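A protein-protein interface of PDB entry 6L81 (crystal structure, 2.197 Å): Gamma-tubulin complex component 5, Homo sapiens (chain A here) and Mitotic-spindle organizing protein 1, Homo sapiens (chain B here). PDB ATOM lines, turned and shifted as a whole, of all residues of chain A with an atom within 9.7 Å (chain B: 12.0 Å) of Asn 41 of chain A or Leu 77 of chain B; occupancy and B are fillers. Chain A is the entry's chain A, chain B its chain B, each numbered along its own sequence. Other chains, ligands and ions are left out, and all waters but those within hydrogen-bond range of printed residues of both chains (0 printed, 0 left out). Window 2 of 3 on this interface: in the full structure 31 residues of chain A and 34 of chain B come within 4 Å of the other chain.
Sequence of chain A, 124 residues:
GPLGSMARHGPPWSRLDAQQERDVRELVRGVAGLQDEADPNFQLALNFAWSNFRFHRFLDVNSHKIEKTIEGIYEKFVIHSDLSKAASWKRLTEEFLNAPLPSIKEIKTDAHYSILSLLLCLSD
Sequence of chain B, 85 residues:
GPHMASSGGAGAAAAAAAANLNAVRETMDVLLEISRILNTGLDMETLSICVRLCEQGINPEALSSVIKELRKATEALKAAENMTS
OG1 of Thr 74 of chain B is in hydrogen-bond range of O of Ala 32 of chain A (2.5 Å).
The side-chain amino group of Lys 72 of chain B lies within salt-bridge range of the side-chain carboxylate of Glu 69 of chain B. The side-chain carboxylate (OD1) of Asp 39 of chain A lies within hydrogen-bond range of the backbone NH (N) of Asn 41 of chain A.
Leu 70 of chain B touches Ala 32 of chain A. Leu 77 of chain B touches Asn 41 of chain A (CD2 to ND2, 3.5 Å). Ala 45 of chain A touches Leu 70 of chain B (CB to CD2, 3.7 Å). Phe 48 of chain A touches Glu 69 of chain B. CG1 of Val 66 of chain B touches CB of Ala 49 of chain A, 3.8 Å away.
Asn 41 of chain A touches one residue of chain B. Leu 77 of chain B touches just one residue of chain A: Asn 41 (3.5 Å). Leu 34 of chain A touches none of the printed residues of chain B. No residue of chain B comes within 4 Å of Asp 39 of chain A. No residue of chain B comes within 4 Å of Phe 42 of chain A. Ala 45 of chain A touches just one residue of chain B: Leu 70 (3.7 Å). Ala 76 of chain B touches none of the printed residues of chain A. Of the printed residues of chain A, Thr 74 of chain B touches Ala 32 (2.5 Å). Printed residues of chain A within 4 Å of Leu 70 of chain B: Ala 32 and Ala 45. Of the printed residues of chain B, Ala 49 of chain A touches Val 66. Of the printed residues of chain B, Phe 48 of chain A touches Glu 69. Val 28 of chain A touches none of the printed residues of chain B. Gln 35 of chain A touches none of the printed residues of chain B. The nearest residue of chain B that does not touch Asn 41 of chain A is Leu 70 of chain B (6.9 Å). The nearest residue of chain A that does not touch Leu 77 of chain B is Leu 34 of chain A (5.1 Å).
Hydrophobic or aromatic side chains of chain A within 4 Å of the printed part of chain B: Ala 32, Ala 45, Phe 48 and Ala 49.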
ATOM      1  N   ARG A  25     -19.189 -34.333  -4.306  1.00  0.00           N
ATOM      2  CA  ARG A  25     -20.090 -33.790  -3.288  1.00  0.00           C
ATOM      3  C   ARG A  25     -19.327 -33.407  -2.031  1.00  0.00           C
ATOM      4  O   ARG A  25     -19.537 -32.326  -1.474  1.00  0.00           O
ATOM      5  CB  ARG A  25     -21.215 -34.784  -2.950  1.00  0.00           C
ATOM      6  CG  ARG A  25     -22.158 -35.052  -4.120  1.00  0.00           C
ATOM      7  CD  ARG A  25     -23.259 -36.081  -3.800  1.00  0.00           C
ATOM      8  NE  ARG A  25     -24.593 -35.516  -3.998  1.00  0.00           N
ATOM      9  CZ  ARG A  25     -25.196 -35.417  -5.185  1.00  0.00           C
ATOM     10  NH1 ARG A  25     -24.581 -35.823  -6.298  1.00  0.00           N
ATOM     11  NH2 ARG A  25     -26.412 -34.891  -5.265  1.00  0.00           N
ATOM     12  N   VAL A  28     -17.464 -30.222  -2.441  1.00  0.00           N
ATOM     13  CA  VAL A  28     -18.316 -29.041  -2.314  1.00  0.00           C
ATOM     14  C   VAL A  28     -18.611 -28.744  -0.842  1.00  0.00           C
ATOM     15  O   VAL A  28     -18.379 -27.628  -0.360  1.00  0.00           O
ATOM     16  CB  VAL A  28     -19.611 -29.234  -3.126  1.00  0.00           C
ATOM     17  CG1 VAL A  28     -20.664 -28.186  -2.739  1.00  0.00           C
ATOM     18  CG2 VAL A  28     -19.308 -29.186  -4.624  1.00  0.00           C
ATOM     19  N   ARG A  29     -19.157 -29.726  -0.119  1.00  0.00           N
ATOM     20  CA  ARG A  29     -19.341 -29.593   1.326  1.00  0.00           C
ATOM     21  C   ARG A  29     -18.092 -29.028   1.992  1.00  0.00           C
ATOM     22  O   ARG A  29     -18.145 -28.005   2.680  1.00  0.00           O
ATOM     23  CB  ARG A  29     -19.691 -30.947   1.952  1.00  0.00           C
ATOM     24  CG  ARG A  29     -21.083 -31.458   1.648  1.00  0.00           C
ATOM     25  CD  ARG A  29     -21.554 -32.431   2.729  1.00  0.00           C
ATOM     26  NE  ARG A  29     -21.063 -33.782   2.478  1.00  0.00           N
ATOM     27  CZ  ARG A  29     -21.679 -34.663   1.695  1.00  0.00           C
ATOM     28  NH1 ARG A  29     -22.815 -34.338   1.095  1.00  0.00           N
ATOM     29  NH2 ARG A  29     -21.161 -35.870   1.514  1.00  0.00           N
ATOM     30  N   ALA A  32     -16.628 -25.429   0.043  1.00  0.00           N
ATOM     31  CA  ALA A  32     -17.611 -24.356   0.076  1.00  0.00           C
ATOM     32  C   ALA A  32     -18.372 -24.277   1.398  1.00  0.00           C
ATOM     33  O   ALA A  32     -19.179 -23.362   1.574  1.00  0.00           O
ATOM     34  CB  ALA A  32     -18.598 -24.509  -1.085  1.00  0.00           C
ATOM     35  N   GLY A  33     -18.136 -25.197   2.328  1.00  0.00           N
ATOM     36  CA  GLY A  33     -18.796 -25.112   3.627  1.00  0.00           C
ATOM     37  C   GLY A  33     -20.302 -25.247   3.572  1.00  0.00           C
ATOM     38  O   GLY A  33     -21.008 -24.594   4.350  1.00  0.00           O
ATOM     39  N   LEU A  34     -20.815 -26.075   2.661  1.00  0.00           N
ATOM     40  CA  LEU A  34     -22.253 -26.302   2.498  1.00  0.00           C
ATOM     41  C   LEU A  34     -22.547 -27.759   2.847  1.00  0.00           C
ATOM     42  O   LEU A  34     -22.497 -28.638   1.984  1.00  0.00           O
ATOM     43  CB  LEU A  34     -22.713 -25.962   1.081  1.00  0.00           C
ATOM     44  CG  LEU A  34     -22.714 -24.475   0.728  1.00  0.00           C
ATOM     45  CD1 LEU A  34     -23.001 -24.275  -0.737  1.00  0.00           C
ATOM     46  CD2 LEU A  34     -23.724 -23.724   1.568  1.00  0.00           C
ATOM     47  N   GLN A  35     -22.874 -28.004   4.114  1.00  0.00           N
ATOM     48  CA  GLN A  35     -23.009 -29.353   4.647  1.00  0.00           C
ATOM     49  C   GLN A  35     -24.406 -29.937   4.476  1.00  0.00           C
ATOM     50  O   GLN A  35     -24.621 -31.095   4.850  1.00  0.00           O
ATOM     51  CB  GLN A  35     -22.622 -29.375   6.135  1.00  0.00           C
ATOM     52  CG  GLN A  35     -21.174 -28.991   6.432  1.00  0.00           C
ATOM     53  CD  GLN A  35     -20.962 -27.486   6.493  1.00  0.00           C
ATOM     54  OE1 GLN A  35     -21.756 -26.717   5.953  1.00  0.00           O
ATOM     55  NE2 GLN A  35     -19.883 -27.060   7.146  1.00  0.00           N
ATOM     56  N   ASP A  36     -25.350 -29.185   3.917  1.00  0.00           N
ATOM     57  CA  ASP A  36     -26.739 -29.628   3.775  1.00  0.00           C
ATOM     58  C   ASP A  36     -27.049 -29.732   2.282  1.00  0.00           C
ATOM     59  O   ASP A  36     -27.309 -28.723   1.620  1.00  0.00           O
ATOM     60  CB  ASP A  36     -27.682 -28.667   4.507  1.00  0.00           C
ATOM     61  CG  ASP A  36     -29.151 -28.870   4.143  1.00  0.00           C
ATOM     62  OD1 ASP A  36     -29.542 -30.009   3.797  1.00  0.00           O
ATOM     63  OD2 ASP A  36     -29.922 -27.884   4.238  1.00  0.00           O
ATOM     64  N   GLU A  37     -27.047 -30.967   1.760  1.00  0.00           N
ATOM     65  CA  GLU A  37     -27.271 -31.185   0.332  1.00  0.00           C
ATOM     66  C   GLU A  37     -28.647 -30.713  -0.131  1.00  0.00           C
ATOM     67  O   GLU A  37     -28.832 -30.474  -1.328  1.00  0.00           O
ATOM     68  CB  GLU A  37     -27.090 -32.664  -0.022  1.00  0.00           C
ATOM     69  CG  GLU A  37     -25.680 -33.198   0.186  1.00  0.00           C
ATOM     70  CD  GLU A  37     -25.437 -34.517  -0.538  1.00  0.00           C
ATOM     71  OE1 GLU A  37     -26.012 -34.719  -1.629  1.00  0.00           O
ATOM     72  OE2 GLU A  37     -24.670 -35.354  -0.013  1.00  0.00           O
ATOM     73  N   ALA A  38     -29.613 -30.581   0.781  1.00  0.00           N
ATOM     74  CA  ALA A  38     -30.917 -30.013   0.466  1.00  0.00           C
ATOM     75  C   ALA A  38     -30.922 -28.487   0.493  1.00  0.00           C
ATOM     76  O   ALA A  38     -31.998 -27.886   0.567  1.00  0.00           O
ATOM     77  CB  ALA A  38     -31.983 -30.555   1.423  1.00  0.00           C
ATOM     78  N   ASP A  39     -29.758 -27.850   0.467  1.00  0.00           N
ATOM     79  CA  ASP A  39     -29.653 -26.415   0.231  1.00  0.00           C
ATOM     80  C   ASP A  39     -29.507 -26.182  -1.264  1.00  0.00           C
ATOM     81  O   ASP A  39     -28.600 -26.764  -1.878  1.00  0.00           O
ATOM     82  CB  ASP A  39     -28.443 -25.841   0.975  1.00  0.00           C
ATOM     83  CG  ASP A  39     -28.320 -24.319   0.862  1.00  0.00           C
ATOM     84  OD1 ASP A  39     -29.010 -23.694   0.031  1.00  0.00           O
ATOM     85  OD2 ASP A  39     -27.498 -23.741   1.611  1.00  0.00           O
ATOM     86  N   PRO A  40     -30.374 -25.378  -1.893  1.00  0.00           N
ATOM     87  CA  PRO A  40     -30.194 -25.085  -3.325  1.00  0.00           C
ATOM     88  C   PRO A  40     -28.796 -24.611  -3.669  1.00  0.00           C
ATOM     89  O   PRO A  40     -28.342 -24.829  -4.797  1.00  0.00           O
ATOM     90  CB  PRO A  40     -31.241 -23.995  -3.590  1.00  0.00           C
ATOM     91  CG  PRO A  40     -32.302 -24.276  -2.610  1.00  0.00           C
ATOM     92  CD  PRO A  40     -31.601 -24.758  -1.364  1.00  0.00           C
ATOM     93  N   ASN A  41     -28.091 -23.985  -2.720  1.00  0.00           N
ATOM     94  CA  ASN A  41     -26.725 -23.549  -2.987  1.00  0.00           C
ATOM     95  C   ASN A  41     -25.778 -24.733  -3.097  1.00  0.00           C
ATOM     96  O   ASN A  41     -24.793 -24.669  -3.839  1.00  0.00           O
ATOM     97  CB  ASN A  41     -26.252 -22.578  -1.905  1.00  0.00           C
ATOM     98  CG  ASN A  41     -26.797 -21.171  -2.107  1.00  0.00           C
ATOM     99  OD1 ASN A  41     -27.339 -20.849  -3.164  1.00  0.00           O
ATOM    100  ND2 ASN A  41     -26.661 -20.331  -1.085  1.00  0.00           N
ATOM    101  N   PHE A  42     -26.057 -25.824  -2.386  1.00  0.00           N
ATOM    102  CA  PHE A  42     -25.268 -27.030  -2.598  1.00  0.00           C
ATOM    103  C   PHE A  42     -25.385 -27.506  -4.043  1.00  0.00           C
ATOM    104  O   PHE A  42     -24.372 -27.719  -4.722  1.00  0.00           O
ATOM    105  CB  PHE A  42     -25.693 -28.135  -1.635  1.00  0.00           C
ATOM    106  CG  PHE A  42     -24.905 -29.399  -1.807  1.00  0.00           C
ATOM    107  CD1 PHE A  42     -23.690 -29.563  -1.158  1.00  0.00           C
ATOM    108  CD2 PHE A  42     -25.357 -30.411  -2.639  1.00  0.00           C
ATOM    109  CE1 PHE A  42     -22.944 -30.718  -1.321  1.00  0.00           C
ATOM    110  CE2 PHE A  42     -24.618 -31.568  -2.806  1.00  0.00           C
ATOM    111  CZ  PHE A  42     -23.405 -31.718  -2.145  1.00  0.00           C
ATOM    112  N   GLN A  43     -26.620 -27.669  -4.538  1.00  0.00           N
ATOM    113  CA  GLN A  43     -26.791 -28.197  -5.887  1.00  0.00           C
ATOM    114  C   GLN A  43     -26.230 -27.243  -6.940  1.00  0.00           C
ATOM    115  O   GLN A  43     -25.657 -27.699  -7.939  1.00  0.00           O
ATOM    116  CB  GLN A  43     -28.267 -28.502  -6.162  1.00  0.00           C
ATOM    117  CG  GLN A  43     -28.462 -29.318  -7.429  1.00  0.00           C
ATOM    118  CD  GLN A  43     -27.881 -30.726  -7.316  1.00  0.00           C
ATOM    119  OE1 GLN A  43     -27.979 -31.373  -6.270  1.00  0.00           O
ATOM    120  NE2 GLN A  43     -27.223 -31.182  -8.383  1.00  0.00           N
ATOM    121  N   LEU A  44     -26.361 -25.925  -6.726  1.00  0.00           N
ATOM    122  CA  LEU A  44     -25.768 -24.962  -7.654  1.00  0.00           C
ATOM    123  C   LEU A  44     -24.248 -25.067  -7.677  1.00  0.00           C
ATOM    124  O   LEU A  44     -23.634 -24.967  -8.746  1.00  0.00           O
ATOM    125  CB  LEU A  44     -26.212 -23.536  -7.307  1.00  0.00           C
ATOM    126  CG  LEU A  44     -27.729 -23.359  -7.467  1.00  0.00           C
ATOM    127  CD1 LEU A  44     -28.260 -22.042  -6.952  1.00  0.00           C
ATOM    128  CD2 LEU A  44     -28.109 -23.529  -8.918  1.00  0.00           C
ATOM    129  N   ALA A  45     -23.621 -25.275  -6.514  1.00  0.00           N
ATOM    130  CA  ALA A  45     -22.170 -25.415  -6.487  1.00  0.00           C
ATOM    131  C   ALA A  45     -21.747 -26.700  -7.186  1.00  0.00           C
ATOM    132  O   ALA A  45     -20.756 -26.716  -7.928  1.00  0.00           O
ATOM    133  CB  ALA A  45     -21.662 -25.386  -5.043  1.00  0.00           C
ATOM    134  N   LEU A  46     -22.524 -27.774  -6.983  1.00  0.00           N
ATOM    135  CA  LEU A  46     -22.232 -29.072  -7.587  1.00  0.00           C
ATOM    136  C   LEU A  46     -22.367 -29.024  -9.110  1.00  0.00           C
ATOM    137  O   LEU A  46     -21.488 -29.505  -9.835  1.00  0.00           O
ATOM    138  CB  LEU A  46     -23.169 -30.131  -6.995  1.00  0.00           C
ATOM    139  CG  LEU A  46     -22.829 -31.587  -7.304  1.00  0.00           C
ATOM    140  CD1 LEU A  46     -21.457 -31.907  -6.768  1.00  0.00           C
ATOM    141  CD2 LEU A  46     -23.861 -32.517  -6.678  1.00  0.00           C
ATOM    142  N   ASN A  47     -23.477 -28.469  -9.609  1.00  0.00           N
ATOM    143  CA  ASN A  47     -23.638 -28.298 -11.051  1.00  0.00           C
ATOM    144  C   ASN A  47     -22.483 -27.494 -11.631  1.00  0.00           C
ATOM    145  O   ASN A  47     -21.947 -27.836 -12.690  1.00  0.00           O
ATOM    146  CB  ASN A  47     -24.957 -27.594 -11.373  1.00  0.00           C
ATOM    147  CG  ASN A  47     -26.194 -28.429 -11.019  1.00  0.00           C
ATOM    148  OD1 ASN A  47     -26.111 -29.634 -10.767  1.00  0.00           O
ATOM    149  ND2 ASN A  47     -27.354 -27.774 -11.004  1.00  0.00           N
ATOM    150  N   PHE A  48     -22.085 -26.417 -10.945  1.00  0.00           N
ATOM    151  CA  PHE A  48     -20.936 -25.647 -11.401  1.00  0.00           C
ATOM    152  C   PHE A  48     -19.660 -26.489 -11.409  1.00  0.00           C
ATOM    153  O   PHE A  48     -18.876 -26.423 -12.363  1.00  0.00           O
ATOM    154  CB  PHE A  48     -20.743 -24.411 -10.535  1.00  0.00           C
ATOM    155  CG  PHE A  48     -19.385 -23.793 -10.674  1.00  0.00           C
ATOM    156  CD1 PHE A  48     -19.064 -23.040 -11.795  1.00  0.00           C
ATOM    157  CD2 PHE A  48     -18.419 -23.972  -9.689  1.00  0.00           C
ATOM    158  CE1 PHE A  48     -17.792 -22.464 -11.933  1.00  0.00           C
ATOM    159  CE2 PHE A  48     -17.152 -23.395  -9.816  1.00  0.00           C
ATOM    160  CZ  PHE A  48     -16.835 -22.643 -10.940  1.00  0.00           C
ATOM    161  N   ALA A  49     -19.419 -27.272 -10.351  1.00  0.00           N
ATOM    162  CA  ALA A  49     -18.187 -28.056 -10.318  1.00  0.00           C
ATOM    163  C   ALA A  49     -18.131 -29.012 -11.505  1.00  0.00           C
ATOM    164  O   ALA A  49     -17.142 -29.041 -12.247  1.00  0.00           O
ATOM    165  CB  ALA A  49     -18.060 -28.828  -8.997  1.00  0.00           C
ATOM    166  N   VAL B  66     -12.106 -24.955  -9.882  1.00  0.00           N
ATOM    167  CA  VAL B  66     -13.303 -25.198  -9.079  1.00  0.00           C
ATOM    168  C   VAL B  66     -13.046 -24.860  -7.618  1.00  0.00           C
ATOM    169  O   VAL B  66     -13.877 -24.227  -6.956  1.00  0.00           O
ATOM    170  CB  VAL B  66     -13.763 -26.658  -9.245  1.00  0.00           C
ATOM    171  CG1 VAL B  66     -14.758 -27.041  -8.164  1.00  0.00           C
ATOM    172  CG2 VAL B  66     -14.373 -26.861 -10.613  1.00  0.00           C
ATOM    173  N   LYS B  68     -10.942 -22.815  -6.235  1.00  0.00           N
ATOM    174  CA  LYS B  68     -10.728 -21.400  -5.948  1.00  0.00           C
ATOM    175  C   LYS B  68     -12.046 -20.631  -5.963  1.00  0.00           C
ATOM    176  O   LYS B  68     -12.256 -19.726  -5.144  1.00  0.00           O
ATOM    177  CB  LYS B  68      -9.735 -20.801  -6.949  1.00  0.00           C
ATOM    178  CG  LYS B  68      -8.264 -21.158  -6.697  1.00  0.00           C
ATOM    179  CD  LYS B  68      -7.399 -20.704  -7.886  1.00  0.00           C
ATOM    180  CE  LYS B  68      -5.903 -20.841  -7.626  1.00  0.00           C
ATOM    181  NZ  LYS B  68      -5.113 -20.481  -8.836  1.00  0.00           N
ATOM    182  N   GLU B  69     -12.946 -20.982  -6.885  1.00  0.00           N
ATOM    183  CA  GLU B  69     -14.259 -20.345  -6.929  1.00  0.00           C
ATOM    184  C   GLU B  69     -15.166 -20.803  -5.790  1.00  0.00           C
ATOM    185  O   GLU B  69     -15.902 -19.983  -5.238  1.00  0.00           O
ATOM    186  CB  GLU B  69     -14.907 -20.583  -8.295  1.00  0.00           C
ATOM    187  CG  GLU B  69     -13.961 -20.226  -9.450  1.00  0.00           C
ATOM    188  CD  GLU B  69     -14.128 -18.806  -9.956  1.00  0.00           C
ATOM    189  OE1 GLU B  69     -13.628 -18.502 -11.062  1.00  0.00           O
ATOM    190  OE2 GLU B  69     -14.775 -18.004  -9.253  1.00  0.00           O
ATOM    191  N   LEU B  70     -15.115 -22.079  -5.386  1.00  0.00           N
ATOM    192  CA  LEU B  70     -15.908 -22.498  -4.229  1.00  0.00           C
ATOM    193  C   LEU B  70     -15.443 -21.838  -2.938  1.00  0.00           C
ATOM    194  O   LEU B  70     -16.230 -21.726  -1.984  1.00  0.00           O
ATOM    195  CB  LEU B  70     -15.883 -24.013  -4.036  1.00  0.00           C
ATOM    196  CG  LEU B  70     -16.462 -24.916  -5.120  1.00  0.00           C
ATOM    197  CD1 LEU B  70     -15.986 -26.326  -4.928  1.00  0.00           C
ATOM    198  CD2 LEU B  70     -17.977 -24.824  -5.074  1.00  0.00           C
ATOM    199  N   ARG B  71     -14.168 -21.435  -2.875  1.00  0.00           N
ATOM    200  CA  ARG B  71     -13.687 -20.626  -1.759  1.00  0.00           C
ATOM    201  C   ARG B  71     -14.121 -19.174  -1.900  1.00  0.00           C
ATOM    202  O   ARG B  71     -14.537 -18.554  -0.919  1.00  0.00           O
ATOM    203  CB  ARG B  71     -12.161 -20.671  -1.661  1.00  0.00           C
ATOM    204  CG  ARG B  71     -11.557 -21.983  -1.195  1.00  0.00           C
ATOM    205  CD  ARG B  71     -10.028 -21.980  -1.382  1.00  0.00           C
ATOM    206  NE  ARG B  71      -9.435 -23.174  -0.799  1.00  0.00           N
ATOM    207  CZ  ARG B  71      -8.142 -23.480  -0.818  1.00  0.00           C
ATOM    208  NH1 ARG B  71      -7.269 -22.674  -1.395  1.00  0.00           N
ATOM    209  NH2 ARG B  71      -7.727 -24.602  -0.248  1.00  0.00           N
ATOM    210  N   LYS B  72     -14.004 -18.616  -3.108  1.00  0.00           N
ATOM    211  CA  LYS B  72     -14.315 -17.207  -3.322  1.00  0.00           C
ATOM    212  C   LYS B  72     -15.759 -16.872  -3.004  1.00  0.00           C
ATOM    213  O   LYS B  72     -16.071 -15.705  -2.743  1.00  0.00           O
ATOM    214  CB  LYS B  72     -14.022 -16.802  -4.765  1.00  0.00           C
ATOM    215  CG  LYS B  72     -12.775 -15.974  -4.924  1.00  0.00           C
ATOM    216  CD  LYS B  72     -12.753 -15.282  -6.273  1.00  0.00           C
ATOM    217  CE  LYS B  72     -12.986 -16.275  -7.392  1.00  0.00           C
ATOM    218  NZ  LYS B  72     -13.178 -15.602  -8.709  1.00  0.00           N
ATOM    219  N   ALA B  73     -16.646 -17.859  -3.016  1.00  0.00           N
ATOM    220  CA  ALA B  73     -18.069 -17.618  -2.834  1.00  0.00           C
ATOM    221  C   ALA B  73     -18.611 -18.353  -1.612  1.00  0.00           C
ATOM    222  O   ALA B  73     -19.779 -18.742  -1.583  1.00  0.00           O
ATOM    223  CB  ALA B  73     -18.841 -18.003  -4.097  1.00  0.00           C
ATOM    224  N   THR B  74     -17.778 -18.552  -0.593  1.00  0.00           N
ATOM    225  CA  THR B  74     -18.249 -19.112   0.669  1.00  0.00           C
ATOM    226  C   THR B  74     -18.017 -18.187   1.852  1.00  0.00           C
ATOM    227  O   THR B  74     -18.897 -18.061   2.709  1.00  0.00           O
ATOM    228  CB  THR B  74     -17.601 -20.488   0.943  1.00  0.00           C
ATOM    229  OG1 THR B  74     -18.272 -21.117   2.043  1.00  0.00           O
ATOM    230  CG2 THR B  74     -16.111 -20.378   1.263  1.00  0.00           C
ATOM    231  N   GLU B  75     -16.862 -17.524   1.922  1.00  0.00           N
ATOM    232  CA  GLU B  75     -16.710 -16.413   2.849  1.00  0.00           C
ATOM    233  C   GLU B  75     -17.641 -15.267   2.485  1.00  0.00           C
ATOM    234  O   GLU B  75     -17.966 -14.443   3.346  1.00  0.00           O
ATOM    235  CB  GLU B  75     -15.257 -15.946   2.859  1.00  0.00           C
ATOM    236  CG  GLU B  75     -14.683 -15.743   1.470  1.00  0.00           C
ATOM    237  CD  GLU B  75     -13.191 -15.959   1.431  1.00  0.00           C
ATOM    238  OE1 GLU B  75     -12.637 -16.419   2.451  1.00  0.00           O
ATOM    239  OE2 GLU B  75     -12.572 -15.674   0.384  1.00  0.00           O
ATOM    240  N   ALA B  76     -18.079 -15.212   1.225  1.00  0.00           N
ATOM    241  CA  ALA B  76     -19.070 -14.251   0.766  1.00  0.00           C
ATOM    242  C   ALA B  76     -20.497 -14.658   1.109  1.00  0.00           C
ATOM    243  O   ALA B  76     -21.413 -13.850   0.919  1.00  0.00           O
ATOM    244  CB  ALA B  76     -18.943 -14.055  -0.747  1.00  0.00           C
ATOM    245  N   LEU B  77     -20.712 -15.878   1.595  1.00  0.00           N
ATOM    246  CA  LEU B  77     -22.042 -16.320   2.006  1.00  0.00           C
ATOM    247  C   LEU B  77     -22.135 -16.418   3.524  1.00  0.00           C
ATOM    248  O   LEU B  77     -21.118 -16.525   4.210  1.00  0.00           O
ATOM    249  CB  LEU B  77     -22.387 -17.671   1.374  1.00  0.00           C
ATOM    250  CG  LEU B  77     -23.242 -17.667   0.102  1.00  0.00           C
ATOM    251  CD1 LEU B  77     -22.653 -16.745  -0.959  1.00  0.00           C
ATOM    252  CD2 LEU B  77     -23.405 -19.083  -0.444  1.00  0.00           C
